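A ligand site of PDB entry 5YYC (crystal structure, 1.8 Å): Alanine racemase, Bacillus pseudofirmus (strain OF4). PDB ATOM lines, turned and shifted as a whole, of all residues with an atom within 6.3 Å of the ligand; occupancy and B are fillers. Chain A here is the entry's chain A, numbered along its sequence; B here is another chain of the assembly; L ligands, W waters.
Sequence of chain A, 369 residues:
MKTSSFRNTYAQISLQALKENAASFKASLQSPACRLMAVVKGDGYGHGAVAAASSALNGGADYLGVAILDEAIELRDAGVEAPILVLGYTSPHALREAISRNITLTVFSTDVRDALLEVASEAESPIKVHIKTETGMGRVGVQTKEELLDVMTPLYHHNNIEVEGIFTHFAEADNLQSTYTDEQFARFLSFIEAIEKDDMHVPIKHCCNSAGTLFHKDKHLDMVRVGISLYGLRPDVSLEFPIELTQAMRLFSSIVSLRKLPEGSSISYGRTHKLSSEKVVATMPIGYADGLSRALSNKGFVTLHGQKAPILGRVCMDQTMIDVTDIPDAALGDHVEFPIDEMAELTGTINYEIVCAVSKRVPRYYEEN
NZ of Lys 41 is covalently linked to C5 of the ligand, at 1.2 Å.
An oxygen (O3) of the ligand sits at hydrogen-bond distance from the side-chain hydroxyl (OH) of Tyr 45, at 2.6 Å.
N of Ser 210 is in hydrogen-bond range of O4 of the ligand, at 2.8 Å.
The side-chain hydroxyl (OG) of Ser 210 lies within hydrogen-bond range of an oxygen (O4) of the ligand (2.6 Å).
The side-chain hydroxyl of Tyr 352 sits at hydrogen-bond distance from an oxygen (O5) of the ligand (2.7 Å).
A nitrogen (N1) of the ligand is in hydrogen-bond range of the guanidinium group (NE) of Arg 225 (2.8 Å).
O3 of the ligand is in hydrogen-bond range of N of Ile 228 (2.8 Å).
An oxygen (O4) of the ligand is in hydrogen-bond range of the backbone NH (N) of Gly 227 (3.1 Å).
O1 of the ligand lies within hydrogen-bond range of NH2 of Arg 139, at 3.3 Å.
A nitrogen (N1) of the ligand sits close to a ring nitrogen (ND1) of His 169 (3.4 Å).
The side-chain hydroxyl (OG) of Ser 210 lies within hydrogen-bond range of the backbone NH (N) of Ile 228, at 3.4 Å.
OG of Ser 210 is in hydrogen-bond range of N of Gly 227 (3.3 Å).
N of Ser 229 is in hydrogen-bond range of OG of Ser 210, 3.1 Å away.
ND1 of His 169 sits at hydrogen-bond distance from NH2 of Arg 225 (3.1 Å).
The backbone NH (N) of Arg 225 lies within hydrogen-bond range of the backbone carbonyl oxygen (O) of Cys 208 (2.8 Å).
The guanidinium group (NH2) of Arg 225 sits at hydrogen-bond distance from the backbone carbonyl oxygen (O) of Thr 168 (2.9 Å).
NE2 of His 169 lies within hydrogen-bond range of OH of Tyr 269 of chain B.
The backbone NH (N) of Ala 211 lies close to the side-chain amide oxygen (OD1) of Asn 209 (3.4 Å).
Merely in contact with the ligand: Leu 87 and Asn 209.
Hydrophobic or aromatic side chains within 4 Å of the ligand: Tyr 45, Leu 87, His 169, Ile 228 and Tyr 352.
Of the 24 residues printed, 11 come within 4 Å of the ligand.
The nearest printed residue that does not touch the ligand is Val 39 (4.1 Å).
Water W1 lies within hydrogen-bond range of an oxygen (O1) of the ligand and the side-chain amide nitrogen of Gln 319 of chain B.
Water W4 lies within hydrogen-bond range of O5 of the ligand (2.9 Å), OH of Tyr 269 of chain B (2.9 Å) and ND2 of Asn 209 (2.9 Å).
Water W2 lies within hydrogen-bond range of the side-chain hydroxyl of Tyr 269 of chain B (2.5 Å), the guanidinium group of Arg 139 (2.6 Å) and an oxygen (O1) of the ligand (3.0 Å).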
ATOM      1  N   VAL A  39       7.770  11.784  -4.917  1.00  0.00           N
ATOM      2  CA  VAL A  39       8.524  10.562  -4.712  1.00  0.00           C
ATOM      3  C   VAL A  39       9.221  10.200  -6.025  1.00  0.00           C
ATOM      4  O   VAL A  39       8.576   9.966  -7.040  1.00  0.00           O
ATOM      5  CB  VAL A  39       7.635   9.416  -4.210  1.00  0.00           C
ATOM      6  CG1 VAL A  39       8.457   8.120  -4.017  1.00  0.00           C
ATOM      7  CG2 VAL A  39       6.972   9.823  -2.894  1.00  0.00           C
ATOM      8  N   LYS A  41      12.019   7.916  -6.228  1.00  0.00           N
ATOM      9  CA  LYS A  41      12.771   6.697  -6.154  1.00  0.00           C
ATOM     10  C   LYS A  41      12.770   5.956  -7.469  1.00  0.00           C
ATOM     11  O   LYS A  41      12.062   6.288  -8.332  1.00  0.00           O
ATOM     12  CB  LYS A  41      12.246   5.822  -5.034  1.00  0.00           C
ATOM     13  CG  LYS A  41      10.859   5.323  -5.223  1.00  0.00           C
ATOM     14  CD  LYS A  41      10.276   4.749  -3.953  1.00  0.00           C
ATOM     15  CE  LYS A  41       9.049   3.911  -4.238  1.00  0.00           C
ATOM     16  NZ  LYS A  41       7.827   4.060  -3.408  1.00  0.00           N
ATOM     17  N   TYR A  45      11.079   6.783 -11.104  1.00  0.00           N
ATOM     18  CA  TYR A  45      10.194   5.764 -11.689  1.00  0.00           C
ATOM     19  C   TYR A  45      10.546   5.548 -13.161  1.00  0.00           C
ATOM     20  O   TYR A  45       9.670   5.469 -14.024  1.00  0.00           O
ATOM     21  CB  TYR A  45       8.710   6.170 -11.545  1.00  0.00           C
ATOM     22  CG  TYR A  45       8.122   5.997 -10.151  1.00  0.00           C
ATOM     23  CD1 TYR A  45       8.739   6.532  -9.029  1.00  0.00           C
ATOM     24  CD2 TYR A  45       6.900   5.349  -9.968  1.00  0.00           C
ATOM     25  CE1 TYR A  45       8.170   6.411  -7.768  1.00  0.00           C
ATOM     26  CE2 TYR A  45       6.323   5.205  -8.703  1.00  0.00           C
ATOM     27  CZ  TYR A  45       6.982   5.746  -7.608  1.00  0.00           C
ATOM     28  OH  TYR A  45       6.439   5.608  -6.348  1.00  0.00           O
ATOM     29  N   LEU A  87      13.221   6.987   2.314  1.00  0.00           N
ATOM     30  CA  LEU A  87      12.000   6.336   2.819  1.00  0.00           C
ATOM     31  C   LEU A  87      12.254   4.955   3.395  1.00  0.00           C
ATOM     32  O   LEU A  87      11.502   4.482   4.261  1.00  0.00           O
ATOM     33  CB  LEU A  87      10.963   6.213   1.705  1.00  0.00           C
ATOM     34  CG  LEU A  87      10.400   7.533   1.171  1.00  0.00           C
ATOM     35  CD1 LEU A  87       9.709   7.287  -0.160  1.00  0.00           C
ATOM     36  CD2 LEU A  87       9.445   8.153   2.200  1.00  0.00           C
ATOM     37  N   LYS A 132       9.461   5.536  11.125  1.00  0.00           N
ATOM     38  CA  LYS A 132       8.514   4.679  10.400  1.00  0.00           C
ATOM     39  C   LYS A 132       7.715   3.809  11.350  1.00  0.00           C
ATOM     40  O   LYS A 132       8.292   3.149  12.237  1.00  0.00           O
ATOM     41  CB  LYS A 132       9.227   3.789   9.382  1.00  0.00           C
ATOM     42  CG  LYS A 132       8.294   2.897   8.516  1.00  0.00           C
ATOM     43  CD  LYS A 132       7.407   3.735   7.623  1.00  0.00           C
ATOM     44  CE  LYS A 132       6.309   2.948   6.902  1.00  0.00           C
ATOM     45  NZ  LYS A 132       6.610   1.531   6.563  1.00  0.00           N
ATOM     46  N   ARG A 139       5.760  -4.472   6.201  1.00  0.00           N
ATOM     47  CA  ARG A 139       7.012  -4.249   5.476  1.00  0.00           C
ATOM     48  C   ARG A 139       8.133  -3.821   6.430  1.00  0.00           C
ATOM     49  O   ARG A 139       8.975  -4.630   6.810  1.00  0.00           O
ATOM     50  CB  ARG A 139       6.780  -3.222   4.373  1.00  0.00           C
ATOM     51  CG  ARG A 139       7.999  -2.973   3.490  1.00  0.00           C
ATOM     52  CD  ARG A 139       7.622  -2.256   2.212  1.00  0.00           C
ATOM     53  NE  ARG A 139       7.223  -0.869   2.423  1.00  0.00           N
ATOM     54  CZ  ARG A 139       6.953  -0.020   1.445  1.00  0.00           C
ATOM     55  NH1 ARG A 139       7.004  -0.433   0.178  1.00  0.00           N
ATOM     56  NH2 ARG A 139       6.623   1.242   1.715  1.00  0.00           N
ATOM     57  N   PHE A 167       5.668   8.506  10.146  1.00  0.00           N
ATOM     58  CA  PHE A 167       4.814   8.112   9.042  1.00  0.00           C
ATOM     59  C   PHE A 167       4.474   6.638   9.010  1.00  0.00           C
ATOM     60  O   PHE A 167       5.016   5.839   9.767  1.00  0.00           O
ATOM     61  CB  PHE A 167       5.422   8.547   7.674  1.00  0.00           C
ATOM     62  CG  PHE A 167       6.689   7.825   7.222  1.00  0.00           C
ATOM     63  CD1 PHE A 167       7.923   8.059   7.832  1.00  0.00           C
ATOM     64  CD2 PHE A 167       6.660   7.008   6.086  1.00  0.00           C
ATOM     65  CE1 PHE A 167       9.091   7.435   7.365  1.00  0.00           C
ATOM     66  CE2 PHE A 167       7.815   6.377   5.605  1.00  0.00           C
ATOM     67  CZ  PHE A 167       9.045   6.596   6.243  1.00  0.00           C
ATOM     68  N   THR A 168       3.547   6.321   8.168  1.00  0.00           N
ATOM     69  CA  THR A 168       3.206   4.954   7.836  1.00  0.00           C
ATOM     70  C   THR A 168       2.886   4.860   6.331  1.00  0.00           C
ATOM     71  O   THR A 168       2.883   5.824   5.643  1.00  0.00           O
ATOM     72  CB  THR A 168       2.129   4.291   8.707  1.00  0.00           C
ATOM     73  OG1 THR A 168       2.207   2.884   8.586  1.00  0.00           O
ATOM     74  CG2 THR A 168       0.783   4.759   8.327  1.00  0.00           C
ATOM     75  N   HIS A 169       2.610   3.651   5.886  1.00  0.00           N
ATOM     76  CA  HIS A 169       2.348   3.390   4.484  1.00  0.00           C
ATOM     77  C   HIS A 169       1.173   2.433   4.314  1.00  0.00           C
ATOM     78  O   HIS A 169       1.092   1.486   5.013  1.00  0.00           O
ATOM     79  CB  HIS A 169       3.572   2.799   3.831  1.00  0.00           C
ATOM     80  CG  HIS A 169       3.531   2.789   2.344  1.00  0.00           C
ATOM     81  ND1 HIS A 169       3.529   3.930   1.596  1.00  0.00           N
ATOM     82  CD2 HIS A 169       3.534   1.771   1.457  1.00  0.00           C
ATOM     83  CE1 HIS A 169       3.522   3.623   0.315  1.00  0.00           C
ATOM     84  NE2 HIS A 169       3.499   2.315   0.209  1.00  0.00           N
ATOM     85  N   CYS A 208      -0.115   9.235   3.294  1.00  0.00           N
ATOM     86  CA  CYS A 208      -0.670   9.009   1.943  1.00  0.00           C
ATOM     87  C   CYS A 208       0.352   8.816   0.840  1.00  0.00           C
ATOM     88  O   CYS A 208       1.321   9.560   0.757  1.00  0.00           O
ATOM     89  CB  CYS A 208      -1.571  10.182   1.535  1.00  0.00           C
ATOM     90  SG  CYS A 208      -3.169  10.239   2.355  1.00  0.00           S
ATOM     91  N   ASN A 209       0.108   7.804   0.005  1.00  0.00           N
ATOM     92  CA  ASN A 209       0.760   7.606  -1.290  1.00  0.00           C
ATOM     93  C   ASN A 209      -0.130   8.240  -2.369  1.00  0.00           C
ATOM     94  O   ASN A 209      -1.017   9.030  -2.028  1.00  0.00           O
ATOM     95  CB  ASN A 209       0.975   6.115  -1.569  1.00  0.00           C
ATOM     96  CG  ASN A 209      -0.291   5.296  -1.419  1.00  0.00           C
ATOM     97  OD1 ASN A 209      -1.376   5.833  -1.202  1.00  0.00           O
ATOM     98  ND2 ASN A 209      -0.159   3.978  -1.532  1.00  0.00           N
ATOM     99  N   SER A 210       0.080   7.937  -3.650  1.00  0.00           N
ATOM    100  CA  SER A 210      -0.791   8.520  -4.691  1.00  0.00           C
ATOM    101  C   SER A 210      -2.267   8.230  -4.436  1.00  0.00           C
ATOM    102  O   SER A 210      -3.116   9.126  -4.491  1.00  0.00           O
ATOM    103  CB  SER A 210      -0.420   8.013  -6.092  1.00  0.00           C
ATOM    104  OG  SER A 210       0.852   8.482  -6.509  1.00  0.00           O
ATOM    105  N   ALA A 211      -2.584   6.957  -4.184  1.00  0.00           N
ATOM    106  CA  ALA A 211      -3.984   6.574  -3.983  1.00  0.00           C
ATOM    107  C   ALA A 211      -4.572   7.245  -2.738  1.00  0.00           C
ATOM    108  O   ALA A 211      -5.707   7.721  -2.752  1.00  0.00           O
ATOM    109  CB  ALA A 211      -4.101   5.034  -3.884  1.00  0.00           C
ATOM    110  N   ARG A 225       2.782  11.817  -0.023  1.00  0.00           N
ATOM    111  CA  ARG A 225       3.942  11.286  -0.734  1.00  0.00           C
ATOM    112  C   ARG A 225       3.484  10.725  -2.080  1.00  0.00           C
ATOM    113  O   ARG A 225       3.076   9.564  -2.177  1.00  0.00           O
ATOM    114  CB  ARG A 225       4.660  10.203   0.089  1.00  0.00           C
ATOM    115  CG  ARG A 225       4.990  10.640   1.528  1.00  0.00           C
ATOM    116  CD  ARG A 225       5.842   9.600   2.263  1.00  0.00           C
ATOM    117  NE  ARG A 225       5.190   8.285   2.238  1.00  0.00           N
ATOM    118  CZ  ARG A 225       4.333   7.863   3.162  1.00  0.00           C
ATOM    119  NH1 ARG A 225       3.993   8.662   4.183  1.00  0.00           N
ATOM    120  NH2 ARG A 225       3.787   6.663   3.052  1.00  0.00           N
ATOM    121  N   VAL A 226       3.564  11.550  -3.110  1.00  0.00           N
ATOM    122  CA  VAL A 226       3.025  11.183  -4.418  1.00  0.00           C
ATOM    123  C   VAL A 226       4.113  10.646  -5.336  1.00  0.00           C
ATOM    124  O   VAL A 226       5.040  11.376  -5.722  1.00  0.00           O
ATOM    125  CB  VAL A 226       2.325  12.380  -5.083  1.00  0.00           C
ATOM    126  CG1 VAL A 226       1.804  12.014  -6.467  1.00  0.00           C
ATOM    127  CG2 VAL A 226       1.182  12.861  -4.187  1.00  0.00           C
ATOM    128  N   GLY A 227       3.975   9.371  -5.716  1.00  0.00           N
ATOM    129  CA  GLY A 227       4.888   8.713  -6.628  1.00  0.00           C
ATOM    130  C   GLY A 227       4.237   8.487  -7.990  1.00  0.00           C
ATOM    131  O   GLY A 227       4.268   9.384  -8.836  1.00  0.00           O
ATOM    132  N   ILE A 228       3.607   7.336  -8.178  1.00  0.00           N
ATOM    133  CA  ILE A 228       3.161   6.909  -9.514  1.00  0.00           C
ATOM    134  C   ILE A 228       2.323   7.965 -10.256  1.00  0.00           C
ATOM    135  O   ILE A 228       2.498   8.168 -11.469  1.00  0.00           O
ATOM    136  CB  ILE A 228       2.360   5.557  -9.426  1.00  0.00           C
ATOM    137  CG1 ILE A 228       2.149   4.950 -10.832  1.00  0.00           C
ATOM    138  CG2 ILE A 228       1.018   5.733  -8.672  1.00  0.00           C
ATOM    139  CD1 ILE A 228       3.461   4.440 -11.522  1.00  0.00           C
ATOM    140  N   SER A 229       1.448   8.688  -9.543  1.00  0.00           N
ATOM    141  CA  SER A 229       0.559   9.621 -10.234  1.00  0.00           C
ATOM    142  C   SER A 229       1.227  10.983 -10.495  1.00  0.00           C
ATOM    143  O   SER A 229       0.703  11.793 -11.274  1.00  0.00           O
ATOM    144  CB  SER A 229      -0.746   9.778  -9.447  1.00  0.00           C
ATOM    145  OG  SER A 229      -1.419   8.516  -9.437  1.00  0.00           O
ATOM    146  N   PRO A 235      -2.605   4.502  -9.920  1.00  0.00           N
ATOM    147  CA  PRO A 235      -2.215   3.492  -8.929  1.00  0.00           C
ATOM    148  C   PRO A 235      -2.779   2.125  -9.288  1.00  0.00           C
ATOM    149  O   PRO A 235      -2.133   1.102  -9.054  1.00  0.00           O
ATOM    150  CB  PRO A 235      -2.843   4.007  -7.628  1.00  0.00           C
ATOM    151  CG  PRO A 235      -3.052   5.463  -7.861  1.00  0.00           C
ATOM    152  CD  PRO A 235      -3.365   5.612  -9.319  1.00  0.00           C
ATOM    153  N   TYR A 352       3.883   0.575 -12.705  1.00  0.00           N
ATOM    154  CA  TYR A 352       5.100   0.849 -11.937  1.00  0.00           C
ATOM    155  C   TYR A 352       6.294   0.040 -12.453  1.00  0.00           C
ATOM    156  O   TYR A 352       7.385   0.570 -12.644  1.00  0.00           O
ATOM    157  CB  TYR A 352       4.960   0.472 -10.466  1.00  0.00           C
ATOM    158  CG  TYR A 352       3.950   1.163  -9.581  1.00  0.00           C
ATOM    159  CD1 TYR A 352       2.591   0.905  -9.699  1.00  0.00           C
ATOM    160  CD2 TYR A 352       4.372   1.982  -8.537  1.00  0.00           C
ATOM    161  CE1 TYR A 352       1.671   1.488  -8.830  1.00  0.00           C
ATOM    162  CE2 TYR A 352       3.458   2.569  -7.661  1.00  0.00           C
ATOM    163  CZ  TYR A 352       2.122   2.317  -7.818  1.00  0.00           C
ATOM    164  OH  TYR A 352       1.208   2.894  -6.952  1.00  0.00           O
ATOM    165  N   TYR B 269       1.468  -5.075  -0.597  1.00  0.00           N
ATOM    166  CA  TYR B 269       0.340  -4.456  -1.301  1.00  0.00           C
ATOM    167  C   TYR B 269      -0.789  -5.420  -1.612  1.00  0.00           C
ATOM    168  O   TYR B 269      -0.533  -6.560  -1.976  1.00  0.00           O
ATOM    169  CB  TYR B 269       0.798  -3.829  -2.611  1.00  0.00           C
ATOM    170  CG  TYR B 269       1.653  -2.599  -2.455  1.00  0.00           C
ATOM    171  CD1 TYR B 269       1.144  -1.438  -1.896  1.00  0.00           C
ATOM    172  CD2 TYR B 269       2.962  -2.585  -2.924  1.00  0.00           C
ATOM    173  CE1 TYR B 269       1.914  -0.303  -1.773  1.00  0.00           C
ATOM    174  CE2 TYR B 269       3.742  -1.451  -2.810  1.00  0.00           C
ATOM    175  CZ  TYR B 269       3.216  -0.312  -2.238  1.00  0.00           C
ATOM    176  OH  TYR B 269       4.001   0.797  -2.159  1.00  0.00           O
ATOM    177  N   MET B 317       8.589  -1.960  -5.133  1.00  0.00           N
ATOM    178  CA  MET B 317       9.615  -1.325  -5.942  1.00  0.00           C
ATOM    179  C   MET B 317      11.022  -1.527  -5.360  1.00  0.00           C
ATOM    180  O   MET B 317      11.966  -1.732  -6.123  1.00  0.00           O
ATOM    181  CB  MET B 317       9.331   0.180  -6.116  1.00  0.00           C
ATOM    182  CG  MET B 317      10.290   0.866  -7.080  1.00  0.00           C
ATOM    183  SD  MET B 317       9.853   2.560  -7.584  1.00  0.00           S
ATOM    184  CE  MET B 317       8.163   2.233  -7.972  1.00  0.00           C
ATOM    185  N   ASP B 318      11.155  -1.459  -4.032  1.00  0.00           N
ATOM    186  CA  ASP B 318      12.472  -1.398  -3.397  1.00  0.00           C
ATOM    187  C   ASP B 318      12.642  -2.411  -2.258  1.00  0.00           C
ATOM    188  O   ASP B 318      13.733  -2.499  -1.671  1.00  0.00           O
ATOM    189  CB  ASP B 318      12.744   0.003  -2.826  1.00  0.00           C
ATOM    190  CG  ASP B 318      12.172   1.094  -3.688  1.00  0.00           C
ATOM    191  OD1 ASP B 318      12.598   1.244  -4.846  1.00  0.00           O
ATOM    192  OD2 ASP B 318      11.280   1.816  -3.207  1.00  0.00           O
ATOM    193  N   GLN B 319      11.572  -3.098  -1.889  1.00  0.00           N
ATOM    194  CA  GLN B 319      11.602  -3.971  -0.720  1.00  0.00           C
ATOM    195  C   GLN B 319      10.829  -5.248  -1.003  1.00  0.00           C
ATOM    196  O   GLN B 319       9.852  -5.239  -1.743  1.00  0.00           O
ATOM    197  CB  GLN B 319      10.989  -3.262   0.514  1.00  0.00           C
ATOM    198  CG  GLN B 319      11.199  -1.751   0.576  1.00  0.00           C
ATOM    199  CD  GLN B 319      11.071  -1.163   1.986  1.00  0.00           C
ATOM    200  OE1 GLN B 319      11.249  -1.840   2.992  1.00  0.00           O
ATOM    201  NE2 GLN B 319      10.678   0.116   2.043  1.00  0.00           N
HETATM  202  N1  LIG L   1       5.645   6.315   0.301  1.00  0.00           N
HETATM  203  C1  LIG L   1       6.436   5.273   0.454  1.00  0.00           C
HETATM  204  C2  LIG L   1       7.015   4.868   1.779  1.00  0.00           C
HETATM  205  C3  LIG L   1       6.789   4.460  -0.689  1.00  0.00           C
HETATM  206  O1  LIG L   1       7.555   3.402  -0.593  1.00  0.00           O
HETATM  207  C4  LIG L   1       6.236   4.835  -1.980  1.00  0.00           C
HETATM  208  C5  LIG L   1       6.600   4.052  -3.178  1.00  0.00           C
HETATM  209  C6  LIG L   1       5.387   6.013  -2.031  1.00  0.00           C
HETATM  210  C7  LIG L   1       5.127   6.673  -0.854  1.00  0.00           C
HETATM  211  C8  LIG L   1       4.760   6.386  -3.354  1.00  0.00           C
HETATM  212  O2  LIG L   1       3.761   5.448  -3.712  1.00  0.00           O
HETATM  213  P1  LIG L   1       2.904   5.621  -5.027  1.00  0.00           P
HETATM  214  O3  LIG L   1       3.861   5.498  -6.061  1.00  0.00           O
HETATM  215  O4  LIG L   1       2.319   6.889  -5.004  1.00  0.00           O
HETATM  216  O5  LIG L   1       1.911   4.633  -5.075  1.00  0.00           O
HETATM  217  O   HOH W   1       9.743   2.935   0.853  1.00  0.00           O
HETATM  218  O   HOH W   2       6.484   0.902  -1.933  1.00  0.00           O
HETATM  219  O   HOH W   3      -0.772   4.792  -4.709  1.00  0.00           O
HETATM  220  O   HOH W   4       1.973   2.650  -3.010  1.00  0.00           O
